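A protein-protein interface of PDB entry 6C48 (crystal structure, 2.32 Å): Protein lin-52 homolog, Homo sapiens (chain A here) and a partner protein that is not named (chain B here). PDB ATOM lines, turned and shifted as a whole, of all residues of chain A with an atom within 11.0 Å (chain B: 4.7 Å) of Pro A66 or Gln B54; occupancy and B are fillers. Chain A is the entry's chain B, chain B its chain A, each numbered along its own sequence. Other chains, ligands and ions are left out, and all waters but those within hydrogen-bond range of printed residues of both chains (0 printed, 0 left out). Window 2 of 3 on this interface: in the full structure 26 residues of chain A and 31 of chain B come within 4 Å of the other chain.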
ATOM      1  N   GLY A  57      -2.350   8.975  28.415  1.00  0.00           N
ATOM      2  CA  GLY A  57      -3.717   9.431  28.593  1.00  0.00           C
ATOM      3  C   GLY A  57      -4.612   8.368  29.188  1.00  0.00           C
ATOM      4  O   GLY A  57      -5.536   8.688  29.943  1.00  0.00           O
ATOM      5  N   LYS A  58      -4.366   7.098  28.847  1.00  0.00           N
ATOM      6  CA  LYS A  58      -5.177   6.009  29.384  1.00  0.00           C
ATOM      7  C   LYS A  58      -5.080   5.955  30.906  1.00  0.00           C
ATOM      8  O   LYS A  58      -6.095   5.899  31.608  1.00  0.00           O
ATOM      9  CB  LYS A  58      -4.743   4.683  28.755  1.00  0.00           C
ATOM     10  CG  LYS A  58      -5.490   3.466  29.282  1.00  0.00           C
ATOM     11  CD  LYS A  58      -4.667   2.201  29.053  1.00  0.00           C
ATOM     12  CE  LYS A  58      -5.557   0.986  28.889  1.00  0.00           C
ATOM     13  NZ  LYS A  58      -6.138   0.570  30.172  1.00  0.00           N
ATOM     14  N   LEU A  60      -4.253   8.340  32.868  1.00  0.00           N
ATOM     15  CA  LEU A  60      -4.707   9.557  33.508  1.00  0.00           C
ATOM     16  C   LEU A  60      -6.213   9.657  33.465  1.00  0.00           C
ATOM     17  O   LEU A  60      -6.774  10.602  34.031  1.00  0.00           O
ATOM     18  CB  LEU A  60      -4.104  10.803  32.852  1.00  0.00           C
ATOM     19  CG  LEU A  60      -2.610  11.068  33.036  1.00  0.00           C
ATOM     20  CD1 LEU A  60      -2.132  12.023  31.971  1.00  0.00           C
ATOM     21  CD2 LEU A  60      -2.337  11.642  34.409  1.00  0.00           C
ATOM     22  N   ASN A  61      -6.872   8.708  32.797  1.00  0.00           N
ATOM     23  CA  ASN A  61      -8.328   8.614  32.781  1.00  0.00           C
ATOM     24  C   ASN A  61      -8.962   9.904  32.300  1.00  0.00           C
ATOM     25  O   ASN A  61      -9.999  10.329  32.812  1.00  0.00           O
ATOM     26  CB  ASN A  61      -8.870   8.224  34.156  1.00  0.00           C
ATOM     27  CG  ASN A  61      -8.514   6.801  34.518  1.00  0.00           C
ATOM     28  OD1 ASN A  61      -8.930   5.861  33.835  1.00  0.00           O
ATOM     29  ND2 ASN A  61      -7.715   6.630  35.571  1.00  0.00           N
ATOM     30  N   ILE A  62      -8.338  10.524  31.298  1.00  0.00           N
ATOM     31  CA  ILE A  62      -8.889  11.753  30.740  1.00  0.00           C
ATOM     32  C   ILE A  62     -10.244  11.481  30.109  1.00  0.00           C
ATOM     33  O   ILE A  62     -11.143  12.323  30.176  1.00  0.00           O
ATOM     34  CB  ILE A  62      -7.888  12.367  29.734  1.00  0.00           C
ATOM     35  CG1 ILE A  62      -6.624  12.838  30.464  1.00  0.00           C
ATOM     36  CG2 ILE A  62      -8.511  13.521  28.930  1.00  0.00           C
ATOM     37  CD1 ILE A  62      -5.427  13.065  29.544  1.00  0.00           C
ATOM     38  N   LEU A  63     -10.439  10.290  29.536  1.00  0.00           N
ATOM     39  CA  LEU A  63     -11.648   9.991  28.773  1.00  0.00           C
ATOM     40  C   LEU A  63     -12.651   9.131  29.539  1.00  0.00           C
ATOM     41  O   LEU A  63     -13.472   8.449  28.915  1.00  0.00           O
ATOM     42  CB  LEU A  63     -11.298   9.320  27.441  1.00  0.00           C
ATOM     43  CG  LEU A  63     -10.478  10.149  26.437  1.00  0.00           C
ATOM     44  CD1 LEU A  63     -10.228   9.398  25.111  1.00  0.00           C
ATOM     45  CD2 LEU A  63     -11.122  11.496  26.183  1.00  0.00           C
ATOM     46  N   GLU A  64     -12.628   9.150  30.867  1.00  0.00           N
ATOM     47  CA  GLU A  64     -13.731   8.559  31.616  1.00  0.00           C
ATOM     48  C   GLU A  64     -14.908   9.534  31.628  1.00  0.00           C
ATOM     49  O   GLU A  64     -14.723  10.750  31.729  1.00  0.00           O
ATOM     50  CB  GLU A  64     -13.310   8.232  33.055  1.00  0.00           C
ATOM     51  CG  GLU A  64     -14.483   7.732  33.918  1.00  0.00           C
ATOM     52  CD  GLU A  64     -14.154   7.575  35.408  1.00  0.00           C
ATOM     53  OE1 GLU A  64     -15.089   7.733  36.231  1.00  0.00           O
ATOM     54  OE2 GLU A  64     -13.009   7.183  35.751  1.00  0.00           O
ATOM     55  N   LYS A  65     -16.119   9.002  31.488  1.00  0.00           N
ATOM     56  CA  LYS A  65     -17.298   9.853  31.536  1.00  0.00           C
ATOM     57  C   LYS A  65     -17.512  10.379  32.957  1.00  0.00           C
ATOM     58  O   LYS A  65     -17.136   9.727  33.937  1.00  0.00           O
ATOM     59  CB  LYS A  65     -18.538   9.096  31.065  1.00  0.00           C
ATOM     60  CG  LYS A  65     -18.344   8.327  29.748  1.00  0.00           C
ATOM     61  CD  LYS A  65     -18.073   6.843  30.008  1.00  0.00           C
ATOM     62  CE  LYS A  65     -17.867   6.071  28.710  1.00  0.00           C
ATOM     63  NZ  LYS A  65     -16.429   5.966  28.344  1.00  0.00           N
ATOM     64  N   PRO A  66     -18.057  11.584  33.095  1.00  0.00           N
ATOM     65  CA  PRO A  66     -18.462  12.052  34.430  1.00  0.00           C
ATOM     66  C   PRO A  66     -19.483  11.109  35.052  1.00  0.00           C
ATOM     67  O   PRO A  66     -20.407  10.635  34.384  1.00  0.00           O
ATOM     68  CB  PRO A  66     -19.069  13.434  34.163  1.00  0.00           C
ATOM     69  CG  PRO A  66     -18.516  13.882  32.866  1.00  0.00           C
ATOM     70  CD  PRO A  66     -18.047  12.662  32.088  1.00  0.00           C
ATOM     71  N   LYS A  67     -19.281  10.793  36.332  1.00  0.00           N
ATOM     72  CA  LYS A  67     -20.241  10.001  37.084  1.00  0.00           C
ATOM     73  C   LYS A  67     -20.799  10.742  38.283  1.00  0.00           C
ATOM     74  O   LYS A  67     -21.830  10.328  38.817  1.00  0.00           O
ATOM     75  CB  LYS A  67     -19.605   8.693  37.584  1.00  0.00           C
ATOM     76  CG  LYS A  67     -18.617   8.021  36.625  1.00  0.00           C
ATOM     77  CD  LYS A  67     -19.204   7.705  35.244  1.00  0.00           C
ATOM     78  CE  LYS A  67     -18.172   6.963  34.382  1.00  0.00           C
ATOM     79  NZ  LYS A  67     -17.294   6.108  35.227  1.00  0.00           N
ATOM     80  N   LYS A  68     -20.162  11.824  38.709  1.00  0.00           N
ATOM     81  CA  LYS A  68     -20.669  12.648  39.797  1.00  0.00           C
ATOM     82  C   LYS A  68     -20.858  14.058  39.242  1.00  0.00           C
ATOM     83  O   LYS A  68     -21.219  14.977  39.976  1.00  0.00           O
ATOM     84  CB  LYS A  68     -19.702  12.652  40.994  1.00  0.00           C
ATOM     85  CG  LYS A  68     -19.579  11.309  41.686  1.00  0.00           C
ATOM     86  CD  LYS A  68     -18.661  11.362  42.898  1.00  0.00           C
ATOM     87  CE  LYS A  68     -18.840  10.129  43.789  1.00  0.00           C
ATOM     88  NZ  LYS A  68     -18.353  10.298  45.206  1.00  0.00           N
ATOM     89  N   ILE B  49     -11.119  17.549  35.625  1.00  0.00           N
ATOM     90  CA  ILE B  49     -10.925  17.821  34.203  1.00  0.00           C
ATOM     91  C   ILE B  49     -12.203  18.431  33.646  1.00  0.00           C
ATOM     92  O   ILE B  49     -13.291  17.867  33.811  1.00  0.00           O
ATOM     93  CB  ILE B  49     -10.578  16.533  33.431  1.00  0.00           C
ATOM     94  CG1 ILE B  49      -9.471  15.709  34.093  1.00  0.00           C
ATOM     95  CG2 ILE B  49     -10.095  16.890  32.066  1.00  0.00           C
ATOM     96  CD1 ILE B  49      -8.118  16.363  34.066  1.00  0.00           C
ATOM     97  N   SER B  50     -12.079  19.552  32.945  1.00  0.00           N
ATOM     98  CA  SER B  50     -13.266  20.165  32.361  1.00  0.00           C
ATOM     99  C   SER B  50     -13.878  19.259  31.299  1.00  0.00           C
ATOM    100  O   SER B  50     -13.197  18.443  30.663  1.00  0.00           O
ATOM    101  CB  SER B  50     -12.933  21.525  31.746  1.00  0.00           C
ATOM    102  OG  SER B  50     -12.653  21.438  30.363  1.00  0.00           O
ATOM    103  N   ILE B  51     -15.193  19.385  31.140  1.00  0.00           N
ATOM    104  CA  ILE B  51     -15.884  18.676  30.066  1.00  0.00           C
ATOM    105  C   ILE B  51     -15.348  19.104  28.704  1.00  0.00           C
ATOM    106  O   ILE B  51     -15.222  18.283  27.789  1.00  0.00           O
ATOM    107  CB  ILE B  51     -17.406  18.886  30.185  1.00  0.00           C
ATOM    108  CG1 ILE B  51     -17.991  17.857  31.154  1.00  0.00           C
ATOM    109  CG2 ILE B  51     -18.099  18.789  28.832  1.00  0.00           C
ATOM    110  CD1 ILE B  51     -19.254  18.340  31.815  1.00  0.00           C
ATOM    111  N   GLU B  52     -15.031  20.393  28.548  1.00  0.00           N
ATOM    112  CA  GLU B  52     -14.541  20.900  27.268  1.00  0.00           C
ATOM    113  C   GLU B  52     -13.191  20.281  26.910  1.00  0.00           C
ATOM    114  O   GLU B  52     -12.950  19.907  25.753  1.00  0.00           O
ATOM    115  CB  GLU B  52     -14.438  22.426  27.324  1.00  0.00           C
ATOM    116  CG  GLU B  52     -15.775  23.145  27.409  1.00  0.00           C
ATOM    117  CD  GLU B  52     -16.397  23.126  28.816  1.00  0.00           C
ATOM    118  OE1 GLU B  52     -15.673  22.910  29.811  1.00  0.00           O
ATOM    119  OE2 GLU B  52     -17.627  23.330  28.932  1.00  0.00           O
ATOM    120  N   PHE B  53     -12.303  20.174  27.896  1.00  0.00           N
ATOM    121  CA  PHE B  53     -11.025  19.496  27.726  1.00  0.00           C
ATOM    122  C   PHE B  53     -11.230  18.059  27.257  1.00  0.00           C
ATOM    123  O   PHE B  53     -10.613  17.620  26.278  1.00  0.00           O
ATOM    124  CB  PHE B  53     -10.270  19.562  29.059  1.00  0.00           C
ATOM    125  CG  PHE B  53      -8.876  18.980  29.043  1.00  0.00           C
ATOM    126  CD1 PHE B  53      -8.676  17.614  29.183  1.00  0.00           C
ATOM    127  CD2 PHE B  53      -7.770  19.807  28.988  1.00  0.00           C
ATOM    128  CE1 PHE B  53      -7.414  17.099  29.227  1.00  0.00           C
ATOM    129  CE2 PHE B  53      -6.505  19.295  29.018  1.00  0.00           C
ATOM    130  CZ  PHE B  53      -6.322  17.940  29.143  1.00  0.00           C
ATOM    131  N   GLN B  54     -12.107  17.313  27.938  1.00  0.00           N
ATOM    132  CA  GLN B  54     -12.363  15.931  27.536  1.00  0.00           C
ATOM    133  C   GLN B  54     -12.817  15.858  26.080  1.00  0.00           C
ATOM    134  O   GLN B  54     -12.328  15.035  25.299  1.00  0.00           O
ATOM    135  CB  GLN B  54     -13.420  15.309  28.445  1.00  0.00           C
ATOM    136  CG  GLN B  54     -13.026  15.173  29.893  1.00  0.00           C
ATOM    137  CD  GLN B  54     -14.084  14.437  30.684  1.00  0.00           C
ATOM    138  OE1 GLN B  54     -15.095  15.015  31.063  1.00  0.00           O
ATOM    139  NE2 GLN B  54     -13.879  13.149  30.901  1.00  0.00           N
ATOM    140  N   ARG B  55     -13.757  16.734  25.711  1.00  0.00           N
ATOM    141  CA  ARG B  55     -14.318  16.754  24.366  1.00  0.00           C
ATOM    142  C   ARG B  55     -13.239  17.022  23.328  1.00  0.00           C
ATOM    143  O   ARG B  55     -13.143  16.317  22.322  1.00  0.00           O
ATOM    144  CB  ARG B  55     -15.409  17.823  24.298  1.00  0.00           C
ATOM    145  CG  ARG B  55     -16.124  17.950  22.986  1.00  0.00           C
ATOM    146  CD  ARG B  55     -16.664  19.365  22.806  1.00  0.00           C
ATOM    147  NE  ARG B  55     -17.840  19.359  21.945  1.00  0.00           N
ATOM    148  CZ  ARG B  55     -17.917  19.927  20.743  1.00  0.00           C
ATOM    149  NH1 ARG B  55     -16.872  20.566  20.213  1.00  0.00           N
ATOM    150  NH2 ARG B  55     -19.051  19.843  20.062  1.00  0.00           N
ATOM    151  N   ARG B  56     -12.392  18.022  23.578  1.00  0.00           N
ATOM    152  CA  ARG B  56     -11.339  18.361  22.628  1.00  0.00           C
ATOM    153  C   ARG B  56     -10.351  17.199  22.472  1.00  0.00           C
ATOM    154  O   ARG B  56      -9.975  16.829  21.350  1.00  0.00           O
ATOM    155  CB  ARG B  56     -10.615  19.628  23.091  1.00  0.00           C
ATOM    156  CG  ARG B  56      -9.484  20.060  22.161  1.00  0.00           C
ATOM    157  CD  ARG B  56      -8.720  21.290  22.642  1.00  0.00           C
ATOM    158  NE  ARG B  56      -7.561  21.519  21.775  1.00  0.00           N
ATOM    159  CZ  ARG B  56      -7.617  22.322  20.710  1.00  0.00           C
ATOM    160  NH1 ARG B  56      -8.749  22.973  20.443  1.00  0.00           N
ATOM    161  NH2 ARG B  56      -6.561  22.494  19.924  1.00  0.00           N
ATOM    162  N   TYR B  57      -9.921  16.623  23.606  1.00  0.00           N
ATOM    163  CA  TYR B  57      -9.059  15.443  23.632  1.00  0.00           C
ATOM    164  C   TYR B  57      -9.654  14.270  22.852  1.00  0.00           C
ATOM    165  O   TYR B  57      -8.968  13.637  22.033  1.00  0.00           O
ATOM    166  CB  TYR B  57      -8.832  15.039  25.085  1.00  0.00           C
ATOM    167  CG  TYR B  57      -7.682  14.120  25.305  1.00  0.00           C
ATOM    168  CD1 TYR B  57      -7.781  12.764  25.000  1.00  0.00           C
ATOM    169  CD2 TYR B  57      -6.496  14.591  25.842  1.00  0.00           C
ATOM    170  CE1 TYR B  57      -6.727  11.910  25.208  1.00  0.00           C
ATOM    171  CE2 TYR B  57      -5.429  13.739  26.062  1.00  0.00           C
ATOM    172  CZ  TYR B  57      -5.551  12.401  25.739  1.00  0.00           C
ATOM    173  OH  TYR B  57      -4.498  11.553  25.947  1.00  0.00           O
ATOM    174  N   ALA B  58     -10.919  13.933  23.140  1.00  0.00           N
ATOM    175  CA  ALA B  58     -11.581  12.847  22.420  1.00  0.00           C
ATOM    176  C   ALA B  58     -11.696  13.151  20.925  1.00  0.00           C
ATOM    177  O   ALA B  58     -11.602  12.241  20.098  1.00  0.00           O
ATOM    178  CB  ALA B  58     -12.960  12.579  23.023  1.00  0.00           C
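O of Ile A62 sits at hydrogen-bond distance from NE2 of Gln B54, 2.9 Å away. O of Glu A64 sits at hydrogen-bond distance from NE2 of Gln B54 (2.7 Å).
The side-chain amino group (NZ) of Lys A67 is in salt-bridge range of the side-chain carboxylate (OE1) of Glu A64, at 2.9 Å. The side-chain hydroxyl of Ser B50 lies within hydrogen-bond range of the backbone NH of Phe B53 (2.8 Å).
Gly A57 touches Tyr B57 (CA to OH, 3.5 Å). Phe B53 touches Ile A62. Tyr B57 touches Ile A62. Gln B54 touches Leu A63 (O to CD2, 3.8 Å). Tyr B57 touches Leu A63. Leu A63 touches Ala B58. Pro A66 touches Gln B54.
Printed residues of chain B within 4 Å of Ile A62: Phe B53 (3.8 Å), Gln B54 (2.9 Å) and Tyr B57 (3.5 Å). Printed residues of chain B within 4 Å of Glu A64: Gln B54. Lys A65 touches none of the printed residues of chain B. Pro A66 touches one residue of chain B. No residue of chain A comes within 4 Å of Ile B49. No residue of chain A comes within 4 Å of Ser B50. No residue of chain A comes within 4 Å of Ile B51. Of chain A, only Ile A62 comes within 4 Å of Phe B53. Gln B54 touches four residues of chain A. Arg B55 touches none of the printed residues of chain A.
Of the 11 printed residues of chain A, 5 touch a printed residue of chain B. Hydrophobic or aromatic side chains of chain A that line the printed part of chain B: Ile A62, Leu A63 and Pro A66. Along chain A the printed residues that touch a printed residue of chain B span positions 57 to 66. Printed residues of chain B that touch a printed residue of chain A: Phe B53, Gln B54, Tyr B57 and Ala B58. Among the printed residues, 9 pairs touch across the chains. Among the printed residues, no Asp or Glu carboxylate lies within 4 Å of a Lys or Arg side-chain nitrogen of the other chain.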
